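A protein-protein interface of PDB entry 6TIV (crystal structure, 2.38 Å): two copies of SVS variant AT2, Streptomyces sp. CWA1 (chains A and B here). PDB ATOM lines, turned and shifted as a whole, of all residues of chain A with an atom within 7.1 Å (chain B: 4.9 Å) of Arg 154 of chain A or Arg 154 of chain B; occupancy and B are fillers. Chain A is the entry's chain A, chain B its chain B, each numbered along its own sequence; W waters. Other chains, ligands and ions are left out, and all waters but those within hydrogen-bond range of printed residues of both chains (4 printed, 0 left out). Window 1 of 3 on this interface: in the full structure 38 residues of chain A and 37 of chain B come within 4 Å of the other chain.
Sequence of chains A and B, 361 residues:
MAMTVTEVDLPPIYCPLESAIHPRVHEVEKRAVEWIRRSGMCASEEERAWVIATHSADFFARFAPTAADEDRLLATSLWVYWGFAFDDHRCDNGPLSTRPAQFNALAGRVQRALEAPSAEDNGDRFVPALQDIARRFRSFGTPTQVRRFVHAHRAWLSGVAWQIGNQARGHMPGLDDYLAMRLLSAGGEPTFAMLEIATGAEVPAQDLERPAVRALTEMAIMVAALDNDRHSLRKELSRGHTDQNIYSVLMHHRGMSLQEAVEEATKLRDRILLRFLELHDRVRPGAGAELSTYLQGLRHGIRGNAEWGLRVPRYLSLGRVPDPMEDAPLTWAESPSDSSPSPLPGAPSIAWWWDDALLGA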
ATOM      1  N   ALA A 107      -2.615 -14.690 -16.478  1.00  0.00           N
ATOM      2  CA  ALA A 107      -2.717 -13.464 -15.665  1.00  0.00           C
ATOM      3  C   ALA A 107      -2.955 -12.277 -16.590  1.00  0.00           C
ATOM      4  O   ALA A 107      -3.779 -11.408 -16.262  1.00  0.00           O
ATOM      5  CB  ALA A 107      -1.459 -13.270 -14.842  1.00  0.00           C
ATOM      6  N   GLY A 108      -2.245 -12.259 -17.709  1.00  0.00           N
ATOM      7  CA  GLY A 108      -2.359 -11.208 -18.730  1.00  0.00           C
ATOM      8  C   GLY A 108      -3.720 -11.240 -19.392  1.00  0.00           C
ATOM      9  O   GLY A 108      -4.351 -10.159 -19.443  1.00  0.00           O
ATOM     10  N   GLN A 111      -6.486 -10.384 -16.633  1.00  0.00           N
ATOM     11  CA  GLN A 111      -6.389  -8.953 -16.228  1.00  0.00           C
ATOM     12  C   GLN A 111      -6.910  -8.093 -17.386  1.00  0.00           C
ATOM     13  O   GLN A 111      -7.637  -7.122 -17.102  1.00  0.00           O
ATOM     14  CB  GLN A 111      -4.980  -8.572 -15.784  1.00  0.00           C
ATOM     15  CG  GLN A 111      -4.882  -7.148 -15.297  1.00  0.00           C
ATOM     16  CD  GLN A 111      -5.570  -6.840 -13.981  1.00  0.00           C
ATOM     17  OE1 GLN A 111      -5.878  -7.708 -13.159  1.00  0.00           O
ATOM     18  NE2 GLN A 111      -5.848  -5.558 -13.794  1.00  0.00           N
ATOM     19  N   ARG A 112      -6.602  -8.458 -18.638  1.00  0.00           N
ATOM     20  CA  ARG A 112      -7.069  -7.686 -19.813  1.00  0.00           C
ATOM     21  C   ARG A 112      -8.605  -7.711 -19.853  1.00  0.00           C
ATOM     22  O   ARG A 112      -9.208  -6.636 -20.065  1.00  0.00           O
ATOM     23  CB  ARG A 112      -6.471  -8.199 -21.127  1.00  0.00           C
ATOM     24  CG  ARG A 112      -6.765  -7.295 -22.320  1.00  0.00           C
ATOM     25  CD  ARG A 112      -6.249  -5.874 -22.126  1.00  0.00           C
ATOM     26  NE  ARG A 112      -6.700  -4.953 -23.158  1.00  0.00           N
ATOM     27  CZ  ARG A 112      -6.741  -3.622 -23.043  1.00  0.00           C
ATOM     28  NH1 ARG A 112      -6.314  -3.041 -21.938  1.00  0.00           N
ATOM     29  NH2 ARG A 112      -7.188  -2.874 -24.043  1.00  0.00           N
ATOM     30  N   LEU A 114     -10.679  -7.951 -17.410  1.00  0.00           N
ATOM     31  CA  LEU A 114     -11.201  -7.043 -16.356  1.00  0.00           C
ATOM     32  C   LEU A 114     -11.197  -5.607 -16.868  1.00  0.00           C
ATOM     33  O   LEU A 114     -12.135  -4.904 -16.578  1.00  0.00           O
ATOM     34  CB  LEU A 114     -10.320  -7.181 -15.112  1.00  0.00           C
ATOM     35  CG  LEU A 114     -10.669  -6.272 -13.954  1.00  0.00           C
ATOM     36  CD1 LEU A 114     -12.084  -6.529 -13.472  1.00  0.00           C
ATOM     37  CD2 LEU A 114      -9.674  -6.527 -12.858  1.00  0.00           C
ATOM     38  N   GLU A 115     -10.168  -5.213 -17.618  1.00  0.00           N
ATOM     39  CA  GLU A 115      -9.959  -3.821 -18.113  1.00  0.00           C
ATOM     40  C   GLU A 115     -10.731  -3.550 -19.413  1.00  0.00           C
ATOM     41  O   GLU A 115     -11.104  -2.428 -19.610  1.00  0.00           O
ATOM     42  CB  GLU A 115      -8.461  -3.568 -18.295  1.00  0.00           C
ATOM     43  CG  GLU A 115      -7.703  -3.693 -16.997  1.00  0.00           C
ATOM     44  CD  GLU A 115      -6.292  -3.134 -16.922  1.00  0.00           C
ATOM     45  OE1 GLU A 115      -6.024  -2.056 -17.488  1.00  0.00           O
ATOM     46  OE2 GLU A 115      -5.480  -3.749 -16.204  1.00  0.00           O
ATOM     47  N   ARG A 147     -10.823   1.847 -11.459  1.00  0.00           N
ATOM     48  CA  ARG A 147      -9.366   1.796 -11.741  1.00  0.00           C
ATOM     49  C   ARG A 147      -8.635   1.334 -10.494  1.00  0.00           C
ATOM     50  O   ARG A 147      -7.731   0.488 -10.633  1.00  0.00           O
ATOM     51  CB  ARG A 147      -8.803   3.109 -12.297  1.00  0.00           C
ATOM     52  CG  ARG A 147      -9.134   3.271 -13.774  1.00  0.00           C
ATOM     53  CD  ARG A 147      -8.320   2.328 -14.645  1.00  0.00           C
ATOM     54  NE  ARG A 147      -6.972   2.861 -14.766  1.00  0.00           N
ATOM     55  CZ  ARG A 147      -5.960   2.256 -15.382  1.00  0.00           C
ATOM     56  NH1 ARG A 147      -6.131   1.060 -15.944  1.00  0.00           N
ATOM     57  NH2 ARG A 147      -4.786   2.877 -15.426  1.00  0.00           N
ATOM     58  N   ARG A 148      -9.046   1.788  -9.316  1.00  0.00           N
ATOM     59  CA  ARG A 148      -8.358   1.338  -8.064  1.00  0.00           C
ATOM     60  C   ARG A 148      -8.476  -0.186  -7.921  1.00  0.00           C
ATOM     61  O   ARG A 148      -7.497  -0.785  -7.541  1.00  0.00           O
ATOM     62  CB  ARG A 148      -8.863   2.081  -6.832  1.00  0.00           C
ATOM     63  CG  ARG A 148      -8.573   3.579  -6.883  1.00  0.00           C
ATOM     64  CD  ARG A 148      -9.398   4.366  -5.882  1.00  0.00           C
ATOM     65  NE  ARG A 148      -9.024   5.770  -5.847  1.00  0.00           N
ATOM     66  CZ  ARG A 148      -9.679   6.730  -5.205  1.00  0.00           C
ATOM     67  NH1 ARG A 148     -10.757   6.433  -4.505  1.00  0.00           N
ATOM     68  NH2 ARG A 148      -9.214   7.967  -5.204  1.00  0.00           N
ATOM     69  N   PHE A 149      -9.624  -0.784  -8.235  1.00  0.00           N
ATOM     70  CA  PHE A 149      -9.824  -2.246  -8.083  1.00  0.00           C
ATOM     71  C   PHE A 149      -8.933  -2.962  -9.113  1.00  0.00           C
ATOM     72  O   PHE A 149      -8.224  -3.917  -8.787  1.00  0.00           O
ATOM     73  CB  PHE A 149     -11.295  -2.651  -8.221  1.00  0.00           C
ATOM     74  CG  PHE A 149     -11.478  -4.147  -8.245  1.00  0.00           C
ATOM     75  CD1 PHE A 149     -11.561  -4.871  -7.074  1.00  0.00           C
ATOM     76  CD2 PHE A 149     -11.525  -4.833  -9.441  1.00  0.00           C
ATOM     77  CE1 PHE A 149     -11.708  -6.246  -7.099  1.00  0.00           C
ATOM     78  CE2 PHE A 149     -11.649  -6.213  -9.465  1.00  0.00           C
ATOM     79  CZ  PHE A 149     -11.750  -6.916  -8.296  1.00  0.00           C
ATOM     80  N   VAL A 150      -8.973  -2.473 -10.336  1.00  0.00           N
ATOM     81  CA  VAL A 150      -8.213  -3.016 -11.489  1.00  0.00           C
ATOM     82  C   VAL A 150      -6.731  -3.068 -11.123  1.00  0.00           C
ATOM     83  O   VAL A 150      -6.097  -4.146 -11.345  1.00  0.00           O
ATOM     84  CB  VAL A 150      -8.470  -2.157 -12.738  1.00  0.00           C
ATOM     85  CG1 VAL A 150      -7.386  -2.331 -13.768  1.00  0.00           C
ATOM     86  CG2 VAL A 150      -9.837  -2.452 -13.340  1.00  0.00           C
ATOM     87  N   HIS A 151      -6.183  -1.965 -10.602  1.00  0.00           N
ATOM     88  CA  HIS A 151      -4.746  -1.873 -10.237  1.00  0.00           C
ATOM     89  C   HIS A 151      -4.450  -2.878  -9.131  1.00  0.00           C
ATOM     90  O   HIS A 151      -3.409  -3.553  -9.194  1.00  0.00           O
ATOM     91  CB  HIS A 151      -4.354  -0.448  -9.810  1.00  0.00           C
ATOM     92  CG  HIS A 151      -4.315   0.534 -10.926  1.00  0.00           C
ATOM     93  ND1 HIS A 151      -3.715   0.258 -12.154  1.00  0.00           N
ATOM     94  CD2 HIS A 151      -4.754   1.809 -10.988  1.00  0.00           C
ATOM     95  CE1 HIS A 151      -3.834   1.333 -12.909  1.00  0.00           C
ATOM     96  NE2 HIS A 151      -4.452   2.281 -12.218  1.00  0.00           N
ATOM     97  N   ALA A 152      -5.350  -2.962  -8.162  1.00  0.00           N
ATOM     98  CA  ALA A 152      -5.237  -3.881  -7.011  1.00  0.00           C
ATOM     99  C   ALA A 152      -5.232  -5.347  -7.479  1.00  0.00           C
ATOM    100  O   ALA A 152      -4.415  -6.173  -7.011  1.00  0.00           O
ATOM    101  CB  ALA A 152      -6.369  -3.585  -6.068  1.00  0.00           C
ATOM    102  N   HIS A 153      -6.140  -5.658  -8.359  1.00  0.00           N
ATOM    103  CA  HIS A 153      -6.302  -6.978  -8.999  1.00  0.00           C
ATOM    104  C   HIS A 153      -5.013  -7.363  -9.720  1.00  0.00           C
ATOM    105  O   HIS A 153      -4.590  -8.512  -9.564  1.00  0.00           O
ATOM    106  CB  HIS A 153      -7.497  -6.916  -9.958  1.00  0.00           C
ATOM    107  CG  HIS A 153      -8.031  -8.257 -10.302  1.00  0.00           C
ATOM    108  ND1 HIS A 153      -7.651  -8.919 -11.449  1.00  0.00           N
ATOM    109  CD2 HIS A 153      -8.946  -9.030  -9.675  1.00  0.00           C
ATOM    110  CE1 HIS A 153      -8.325 -10.055 -11.517  1.00  0.00           C
ATOM    111  NE2 HIS A 153      -9.142 -10.140 -10.449  1.00  0.00           N
ATOM    112  N   ARG A 154      -4.370  -6.429 -10.431  1.00  0.00           N
ATOM    113  CA  ARG A 154      -3.100  -6.746 -11.118  1.00  0.00           C
ATOM    114  C   ARG A 154      -2.052  -6.968 -10.032  1.00  0.00           C
ATOM    115  O   ARG A 154      -1.274  -7.931 -10.117  1.00  0.00           O
ATOM    116  CB  ARG A 154      -2.671  -5.685 -12.136  1.00  0.00           C
ATOM    117  CG  ARG A 154      -1.485  -6.158 -12.979  1.00  0.00           C
ATOM    118  CD  ARG A 154      -0.808  -5.151 -13.880  1.00  0.00           C
ATOM    119  NE  ARG A 154      -1.725  -4.371 -14.704  1.00  0.00           N
ATOM    120  CZ  ARG A 154      -2.275  -4.807 -15.825  1.00  0.00           C
ATOM    121  NH1 ARG A 154      -2.037  -6.036 -16.254  1.00  0.00           N
ATOM    122  NH2 ARG A 154      -3.062  -4.016 -16.522  1.00  0.00           N
ATOM    123  N   ALA A 155      -2.030  -6.147  -8.992  1.00  0.00           N
ATOM    124  CA  ALA A 155      -1.042  -6.377  -7.914  1.00  0.00           C
ATOM    125  C   ALA A 155      -1.151  -7.827  -7.401  1.00  0.00           C
ATOM    126  O   ALA A 155      -0.084  -8.495  -7.206  1.00  0.00           O
ATOM    127  CB  ALA A 155      -1.208  -5.352  -6.819  1.00  0.00           C
ATOM    128  N   TRP A 156      -2.381  -8.293  -7.141  1.00  0.00           N
ATOM    129  CA  TRP A 156      -2.610  -9.653  -6.608  1.00  0.00           C
ATOM    130  C   TRP A 156      -2.012 -10.686  -7.577  1.00  0.00           C
ATOM    131  O   TRP A 156      -1.233 -11.549  -7.144  1.00  0.00           O
ATOM    132  CB  TRP A 156      -4.094  -9.867  -6.348  1.00  0.00           C
ATOM    133  CG  TRP A 156      -4.485 -11.300  -6.225  1.00  0.00           C
ATOM    134  CD1 TRP A 156      -3.994 -12.232  -5.370  1.00  0.00           C
ATOM    135  CD2 TRP A 156      -5.483 -11.965  -7.010  1.00  0.00           C
ATOM    136  NE1 TRP A 156      -4.629 -13.426  -5.557  1.00  0.00           N
ATOM    137  CE2 TRP A 156      -5.515 -13.303  -6.587  1.00  0.00           C
ATOM    138  CE3 TRP A 156      -6.302 -11.554  -8.059  1.00  0.00           C
ATOM    139  CZ2 TRP A 156      -6.387 -14.231  -7.132  1.00  0.00           C
ATOM    140  CZ3 TRP A 156      -7.134 -12.482  -8.630  1.00  0.00           C
ATOM    141  CH2 TRP A 156      -7.176 -13.798  -8.171  1.00  0.00           C
ATOM    142  N   LEU A 157      -2.276 -10.554  -8.869  1.00  0.00           N
ATOM    143  CA  LEU A 157      -1.813 -11.557  -9.852  1.00  0.00           C
ATOM    144  C   LEU A 157      -0.289 -11.537  -9.893  1.00  0.00           C
ATOM    145  O   LEU A 157       0.306 -12.653 -10.054  1.00  0.00           O
ATOM    146  CB  LEU A 157      -2.462 -11.298 -11.205  1.00  0.00           C
ATOM    147  CG  LEU A 157      -3.980 -11.538 -11.228  1.00  0.00           C
ATOM    148  CD1 LEU A 157      -4.555 -11.000 -12.499  1.00  0.00           C
ATOM    149  CD2 LEU A 157      -4.355 -13.010 -11.075  1.00  0.00           C
ATOM    150  N   SER A 158       0.330 -10.373  -9.705  1.00  0.00           N
ATOM    151  CA  SER A 158       1.810 -10.273  -9.729  1.00  0.00           C
ATOM    152  C   SER A 158       2.363 -11.129  -8.610  1.00  0.00           C
ATOM    153  O   SER A 158       3.405 -11.765  -8.817  1.00  0.00           O
ATOM    154  CB  SER A 158       2.335  -8.866  -9.618  1.00  0.00           C
ATOM    155  OG  SER A 158       1.998  -8.141 -10.794  1.00  0.00           O
ATOM    156  N   GLY A 159       1.719 -11.077  -7.449  1.00  0.00           N
ATOM    157  CA  GLY A 159       2.135 -11.868  -6.279  1.00  0.00           C
ATOM    158  C   GLY A 159       1.959 -13.344  -6.550  1.00  0.00           C
ATOM    159  O   GLY A 159       2.858 -14.115  -6.188  1.00  0.00           O
ATOM    160  N   VAL A 160       0.817 -13.749  -7.097  1.00  0.00           N
ATOM    161  CA  VAL A 160       0.599 -15.189  -7.413  1.00  0.00           C
ATOM    162  C   VAL A 160       1.714 -15.658  -8.359  1.00  0.00           C
ATOM    163  O   VAL A 160       2.268 -16.761  -8.110  1.00  0.00           O
ATOM    164  CB  VAL A 160      -0.794 -15.482  -7.990  1.00  0.00           C
ATOM    165  CG1 VAL A 160      -0.924 -16.951  -8.339  1.00  0.00           C
ATOM    166  CG2 VAL A 160      -1.895 -15.053  -7.029  1.00  0.00           C
ATOM    167  N   LEU A 184       0.818  -9.358  -1.612  1.00  0.00           N
ATOM    168  CA  LEU A 184       0.104  -9.370  -2.900  1.00  0.00           C
ATOM    169  C   LEU A 184      -0.681 -10.680  -3.118  1.00  0.00           C
ATOM    170  O   LEU A 184      -1.863 -10.599  -3.505  1.00  0.00           O
ATOM    171  CB  LEU A 184       1.133  -9.105  -3.991  1.00  0.00           C
ATOM    172  CG  LEU A 184       1.913  -7.787  -3.923  1.00  0.00           C
ATOM    173  CD1 LEU A 184       2.826  -7.687  -5.121  1.00  0.00           C
ATOM    174  CD2 LEU A 184       1.017  -6.554  -3.873  1.00  0.00           C
ATOM    175  N   GLU A 189      -5.232  -6.770  -1.498  1.00  0.00           N
ATOM    176  CA  GLU A 189      -5.287  -5.498  -2.242  1.00  0.00           C
ATOM    177  C   GLU A 189      -6.622  -5.396  -2.958  1.00  0.00           C
ATOM    178  O   GLU A 189      -7.399  -4.487  -2.703  1.00  0.00           O
ATOM    179  CB  GLU A 189      -4.076  -5.362  -3.168  1.00  0.00           C
ATOM    180  CG  GLU A 189      -2.809  -5.049  -2.419  1.00  0.00           C
ATOM    181  CD  GLU A 189      -2.621  -3.592  -2.023  1.00  0.00           C
ATOM    182  OE1 GLU A 189      -3.538  -2.778  -2.191  1.00  0.00           O
ATOM    183  OE2 GLU A 189      -1.550  -3.281  -1.491  1.00  0.00           O
ATOM    184  N   PRO A 190      -7.004  -6.306  -3.877  1.00  0.00           N
ATOM    185  CA  PRO A 190      -8.317  -6.166  -4.497  1.00  0.00           C
ATOM    186  C   PRO A 190      -9.454  -6.287  -3.469  1.00  0.00           C
ATOM    187  O   PRO A 190     -10.444  -5.662  -3.622  1.00  0.00           O
ATOM    188  CB  PRO A 190      -8.322  -7.277  -5.558  1.00  0.00           C
ATOM    189  CG  PRO A 190      -7.304  -8.279  -5.071  1.00  0.00           C
ATOM    190  CD  PRO A 190      -6.258  -7.476  -4.329  1.00  0.00           C
ATOM    191  N   GLN B 111       9.527  -4.034  -8.189  1.00  0.00           N
ATOM    192  CA  GLN B 111       8.282  -3.276  -7.952  1.00  0.00           C
ATOM    193  C   GLN B 111       8.165  -2.971  -6.448  1.00  0.00           C
ATOM    194  O   GLN B 111       7.828  -1.838  -6.091  1.00  0.00           O
ATOM    195  CB  GLN B 111       7.070  -4.002  -8.536  1.00  0.00           C
ATOM    196  CG  GLN B 111       5.787  -3.223  -8.345  1.00  0.00           C
ATOM    197  CD  GLN B 111       5.638  -2.055  -9.282  1.00  0.00           C
ATOM    198  OE1 GLN B 111       6.335  -1.972 -10.285  1.00  0.00           O
ATOM    199  NE2 GLN B 111       4.667  -1.196  -9.001  1.00  0.00           N
ATOM    200  N   GLU B 115       7.875   0.924  -4.419  1.00  0.00           N
ATOM    201  CA  GLU B 115       6.734   1.239  -3.518  1.00  0.00           C
ATOM    202  C   GLU B 115       7.216   1.451  -2.076  1.00  0.00           C
ATOM    203  O   GLU B 115       6.545   2.174  -1.332  1.00  0.00           O
ATOM    204  CB  GLU B 115       5.716   0.098  -3.602  1.00  0.00           C
ATOM    205  CG  GLU B 115       5.177  -0.157  -5.014  1.00  0.00           C
ATOM    206  CD  GLU B 115       3.796  -0.814  -5.079  1.00  0.00           C
ATOM    207  OE1 GLU B 115       3.494  -1.527  -6.062  1.00  0.00           O
ATOM    208  OE2 GLU B 115       2.987  -0.533  -4.200  1.00  0.00           O
ATOM    209  N   VAL B 150       3.535   4.000 -10.273  1.00  0.00           N
ATOM    210  CA  VAL B 150       3.730   2.671  -9.603  1.00  0.00           C
ATOM    211  C   VAL B 150       2.847   1.615 -10.297  1.00  0.00           C
ATOM    212  O   VAL B 150       3.377   0.551 -10.657  1.00  0.00           O
ATOM    213  CB  VAL B 150       3.399   2.796  -8.101  1.00  0.00           C
ATOM    214  CG1 VAL B 150       3.171   1.453  -7.453  1.00  0.00           C
ATOM    215  CG2 VAL B 150       4.440   3.616  -7.322  1.00  0.00           C
ATOM    216  N   HIS B 151       1.545   1.899 -10.455  1.00  0.00           N
ATOM    217  CA  HIS B 151       0.583   0.987 -11.119  1.00  0.00           C
ATOM    218  C   HIS B 151       0.988   0.781 -12.592  1.00  0.00           C
ATOM    219  O   HIS B 151       0.949  -0.343 -13.065  1.00  0.00           O
ATOM    220  CB  HIS B 151      -0.859   1.503 -11.008  1.00  0.00           C
ATOM    221  CG  HIS B 151      -1.403   1.580  -9.630  1.00  0.00           C
ATOM    222  ND1 HIS B 151      -1.162   0.614  -8.678  1.00  0.00           N
ATOM    223  CD2 HIS B 151      -2.188   2.498  -9.032  1.00  0.00           C
ATOM    224  CE1 HIS B 151      -1.756   0.976  -7.540  1.00  0.00           C
ATOM    225  NE2 HIS B 151      -2.410   2.076  -7.739  1.00  0.00           N
ATOM    226  N   ALA B 152       1.358   1.846 -13.297  1.00  0.00           N
ATOM    227  CA  ALA B 152       1.864   1.768 -14.689  1.00  0.00           C
ATOM    228  C   ALA B 152       3.104   0.869 -14.772  1.00  0.00           C
ATOM    229  O   ALA B 152       3.209   0.082 -15.744  1.00  0.00           O
ATOM    230  CB  ALA B 152       2.167   3.134 -15.206  1.00  0.00           C
ATOM    231  N   HIS B 153       4.011   0.999 -13.811  1.00  0.00           N
ATOM    232  CA  HIS B 153       5.280   0.243 -13.760  1.00  0.00           C
ATOM    233  C   HIS B 153       4.987  -1.248 -13.535  1.00  0.00           C
ATOM    234  O   HIS B 153       5.603  -2.072 -14.232  1.00  0.00           O
ATOM    235  CB  HIS B 153       6.171   0.847 -12.680  1.00  0.00           C
ATOM    236  CG  HIS B 153       7.596   0.440 -12.760  1.00  0.00           C
ATOM    237  ND1 HIS B 153       8.043  -0.751 -12.233  1.00  0.00           N
ATOM    238  CD2 HIS B 153       8.689   1.101 -13.203  1.00  0.00           C
ATOM    239  CE1 HIS B 153       9.357  -0.828 -12.399  1.00  0.00           C
ATOM    240  NE2 HIS B 153       9.785   0.304 -12.965  1.00  0.00           N
ATOM    241  N   ARG B 154       4.053  -1.582 -12.635  1.00  0.00           N
ATOM    242  CA  ARG B 154       3.644  -2.989 -12.421  1.00  0.00           C
ATOM    243  C   ARG B 154       3.000  -3.512 -13.716  1.00  0.00           C
ATOM    244  O   ARG B 154       3.281  -4.640 -14.079  1.00  0.00           O
ATOM    245  CB  ARG B 154       2.744  -3.159 -11.199  1.00  0.00           C
ATOM    246  CG  ARG B 154       2.257  -4.597 -11.044  1.00  0.00           C
ATOM    247  CD  ARG B 154       1.296  -4.902  -9.920  1.00  0.00           C
ATOM    248  NE  ARG B 154       2.106  -4.941  -8.715  1.00  0.00           N
ATOM    249  CZ  ARG B 154       2.107  -4.016  -7.755  1.00  0.00           C
ATOM    250  NH1 ARG B 154       1.290  -2.974  -7.824  1.00  0.00           N
ATOM    251  NH2 ARG B 154       2.924  -4.174  -6.723  1.00  0.00           N
ATOM    252  N   ALA B 155       2.217  -2.714 -14.445  1.00  0.00           N
ATOM    253  CA  ALA B 155       1.553  -3.173 -15.694  1.00  0.00           C
ATOM    254  C   ALA B 155       2.608  -3.562 -16.728  1.00  0.00           C
ATOM    255  O   ALA B 155       2.486  -4.600 -17.379  1.00  0.00           O
ATOM    256  CB  ALA B 155       0.650  -2.102 -16.230  1.00  0.00           C
ATOM    257  N   TRP B 156       3.610  -2.722 -16.881  1.00  0.00           N
ATOM    258  CA  TRP B 156       4.749  -3.005 -17.769  1.00  0.00           C
ATOM    259  C   TRP B 156       5.436  -4.320 -17.352  1.00  0.00           C
ATOM    260  O   TRP B 156       5.624  -5.200 -18.219  1.00  0.00           O
ATOM    261  CB  TRP B 156       5.704  -1.828 -17.761  1.00  0.00           C
ATOM    262  CG  TRP B 156       7.022  -2.123 -18.371  1.00  0.00           C
ATOM    263  CD1 TRP B 156       7.246  -2.479 -19.660  1.00  0.00           C
ATOM    264  CD2 TRP B 156       8.305  -2.030 -17.733  1.00  0.00           C
ATOM    265  NE1 TRP B 156       8.582  -2.632 -19.874  1.00  0.00           N
ATOM    266  CE2 TRP B 156       9.269  -2.350 -18.720  1.00  0.00           C
ATOM    267  CE3 TRP B 156       8.735  -1.714 -16.438  1.00  0.00           C
ATOM    268  CZ2 TRP B 156      10.639  -2.364 -18.453  1.00  0.00           C
ATOM    269  CZ3 TRP B 156      10.091  -1.751 -16.165  1.00  0.00           C
ATOM    270  CH2 TRP B 156      11.026  -2.089 -17.155  1.00  0.00           C
ATOM    271  N   LEU B 157       5.776  -4.472 -16.079  1.00  0.00           N
ATOM    272  CA  LEU B 157       6.415  -5.712 -15.582  1.00  0.00           C
ATOM    273  C   LEU B 157       5.538  -6.930 -15.910  1.00  0.00           C
ATOM    274  O   LEU B 157       6.096  -7.970 -16.342  1.00  0.00           O
ATOM    275  CB  LEU B 157       6.723  -5.560 -14.092  1.00  0.00           C
ATOM    276  CG  LEU B 157       7.877  -4.596 -13.819  1.00  0.00           C
ATOM    277  CD1 LEU B 157       8.056  -4.356 -12.335  1.00  0.00           C
ATOM    278  CD2 LEU B 157       9.188  -5.068 -14.446  1.00  0.00           C
ATOM    279  N   SER B 158       4.227  -6.836 -15.738  1.00  0.00           N
ATOM    280  CA  SER B 158       3.303  -7.948 -16.082  1.00  0.00           C
ATOM    281  C   SER B 158       3.437  -8.286 -17.574  1.00  0.00           C
ATOM    282  O   SER B 158       3.410  -9.496 -17.933  1.00  0.00           O
ATOM    283  CB  SER B 158       1.892  -7.600 -15.720  1.00  0.00           C
ATOM    284  OG  SER B 158       1.786  -7.506 -14.304  1.00  0.00           O
ATOM    285  N   LEU B 184       1.457  -3.504 -22.783  1.00  0.00           N
ATOM    286  CA  LEU B 184       2.135  -3.464 -21.471  1.00  0.00           C
ATOM    287  C   LEU B 184       3.647  -3.591 -21.647  1.00  0.00           C
ATOM    288  O   LEU B 184       4.343  -2.763 -21.105  1.00  0.00           O
ATOM    289  CB  LEU B 184       1.595  -4.608 -20.623  1.00  0.00           C
ATOM    290  CG  LEU B 184       0.106  -4.568 -20.303  1.00  0.00           C
ATOM    291  CD1 LEU B 184      -0.194  -5.619 -19.262  1.00  0.00           C
ATOM    292  CD2 LEU B 184      -0.306  -3.184 -19.787  1.00  0.00           C
HETATM  293  O   HOH W   1       0.250  -9.238 -13.100  1.00  0.00           O
HETATM  294  O   HOH W   2       4.133  -7.730 -12.446  1.00  0.00           O
HETATM  295  O   HOH W   3      -0.909  -2.560  -9.873  1.00  0.00           O
HETATM  296  O   HOH W   4      -1.255  -2.022 -12.542  1.00  0.00           O
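A ring nitrogen (NE2) of His 151 of chain A lies close to the guanidinium group (NH2) of Arg 147 of chain A. The backbone carbonyl oxygen of Arg 154 of chain A sits at hydrogen-bond distance from the side-chain hydroxyl of Ser 158 of chain A (3.3 Å). OE1 of Gln 111 of chain B sits at hydrogen-bond distance from N of Arg 154 of chain B (3.3 Å). O of Arg 154 of chain B is in hydrogen-bond range of OG of Ser 158 of chain B (3.2 Å).
His 151 of chain A touches His 151 of chain B (CD2 to CD2, 3.3 Å). Arg 154 of chain A touches Arg 154 of chain B. Arg 154 of chain A touches Ala 155 of chain B (CD to CA, 3.6 Å). Ser 158 of chain B touches Arg 154 of chain A (OG to CD, 3.5 Å). Leu 184 of chain B touches Arg 154 of chain A. OG of Ser 158 of chain A touches CD of Arg 154 of chain B, at 3.4 Å. Ser 158 of chain A touches Ser 158 of chain B (OG to OG, 3.6 Å). NH2 of Arg 154 of chain B touches CD1 of Leu 184 of chain A, at 3.9 Å.
Ala 107 of chain A touches none of the printed residues of chain B. Leu 114 of chain A touches none of the printed residues of chain B. Of the printed residues of chain B, Arg 154 of chain A touches Arg 154 (3.9 Å), Ala 155 (3.6 Å), Ser 158 (3.5 Å) and Leu 184 (3.6 Å). Printed residues of chain B within 4 Å of Ser 158 of chain A: Arg 154 and Ser 158. Of the printed residues of chain B, Leu 184 of chain A touches Arg 154. Of chain A, only Arg 154, Ala 155, Ser 158 and Leu 184 come within 4 Å of Arg 154 of chain B. Of the printed residues of chain A, Ala 155 of chain B touches Arg 154 (3.6 Å). The nearest printed residue of chain B that does not touch Arg 154 of chain A is His 151 of chain B (5.1 Å). The nearest printed residue of chain A that does not touch Ala 155 of chain B is Glu 115 of chain A (6.3 Å).
Of the 23 printed residues of chain A, 5 touch a printed residue of chain B. Hydrophobic or aromatic side chains of chain A that line the printed part of chain B: His 151, Ala 155 and Leu 184. Of the 12 printed residues of chain B, 5 touch a printed residue of chain A. Hydrophobic or aromatic side chains of chain B that line the printed part of chain A: His 151, Ala 155 and Leu 184. Among the printed residues, 9 pairs touch across the chains. Among the printed residues, no Asp or Glu carboxylate lies within 4 Å of a Lys or Arg side-chain nitrogen of the other chain.
His 151 of chain A touches its own counterpart, His 151 of chain B. Arg 154 of chain A touches its own counterpart, Arg 154 of chain B. Arg 154 of chain A touches Ala 155 of chain B, and with the chains exchanged Ala 155 of chain A touches Arg 154 of chain B. Ser 158 of chain A touches its own counterpart, Ser 158 of chain B. Of the 9 pairs that touch across the chains among the printed residues, 9 have their exchanged pair printed and touching as well.
Water W1 lies within hydrogen-bond range of the side-chain hydroxyl (OG) of Ser 158 of chain B (2.6 Å) and the side-chain hydroxyl (OG) of Ser 158 of chain A (3.1 Å). Water W2 lies within hydrogen-bond range of OG of Ser 158 of chain A (2.7 Å) and OG of Ser 158 of chain B (3.0 Å). Water W3 lies within hydrogen-bond range of the backbone carbonyl oxygen of His 151 of chain A, the guanidinium group of Arg 154 of chain B and a ring nitrogen (ND1) of His 151 of chain B.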
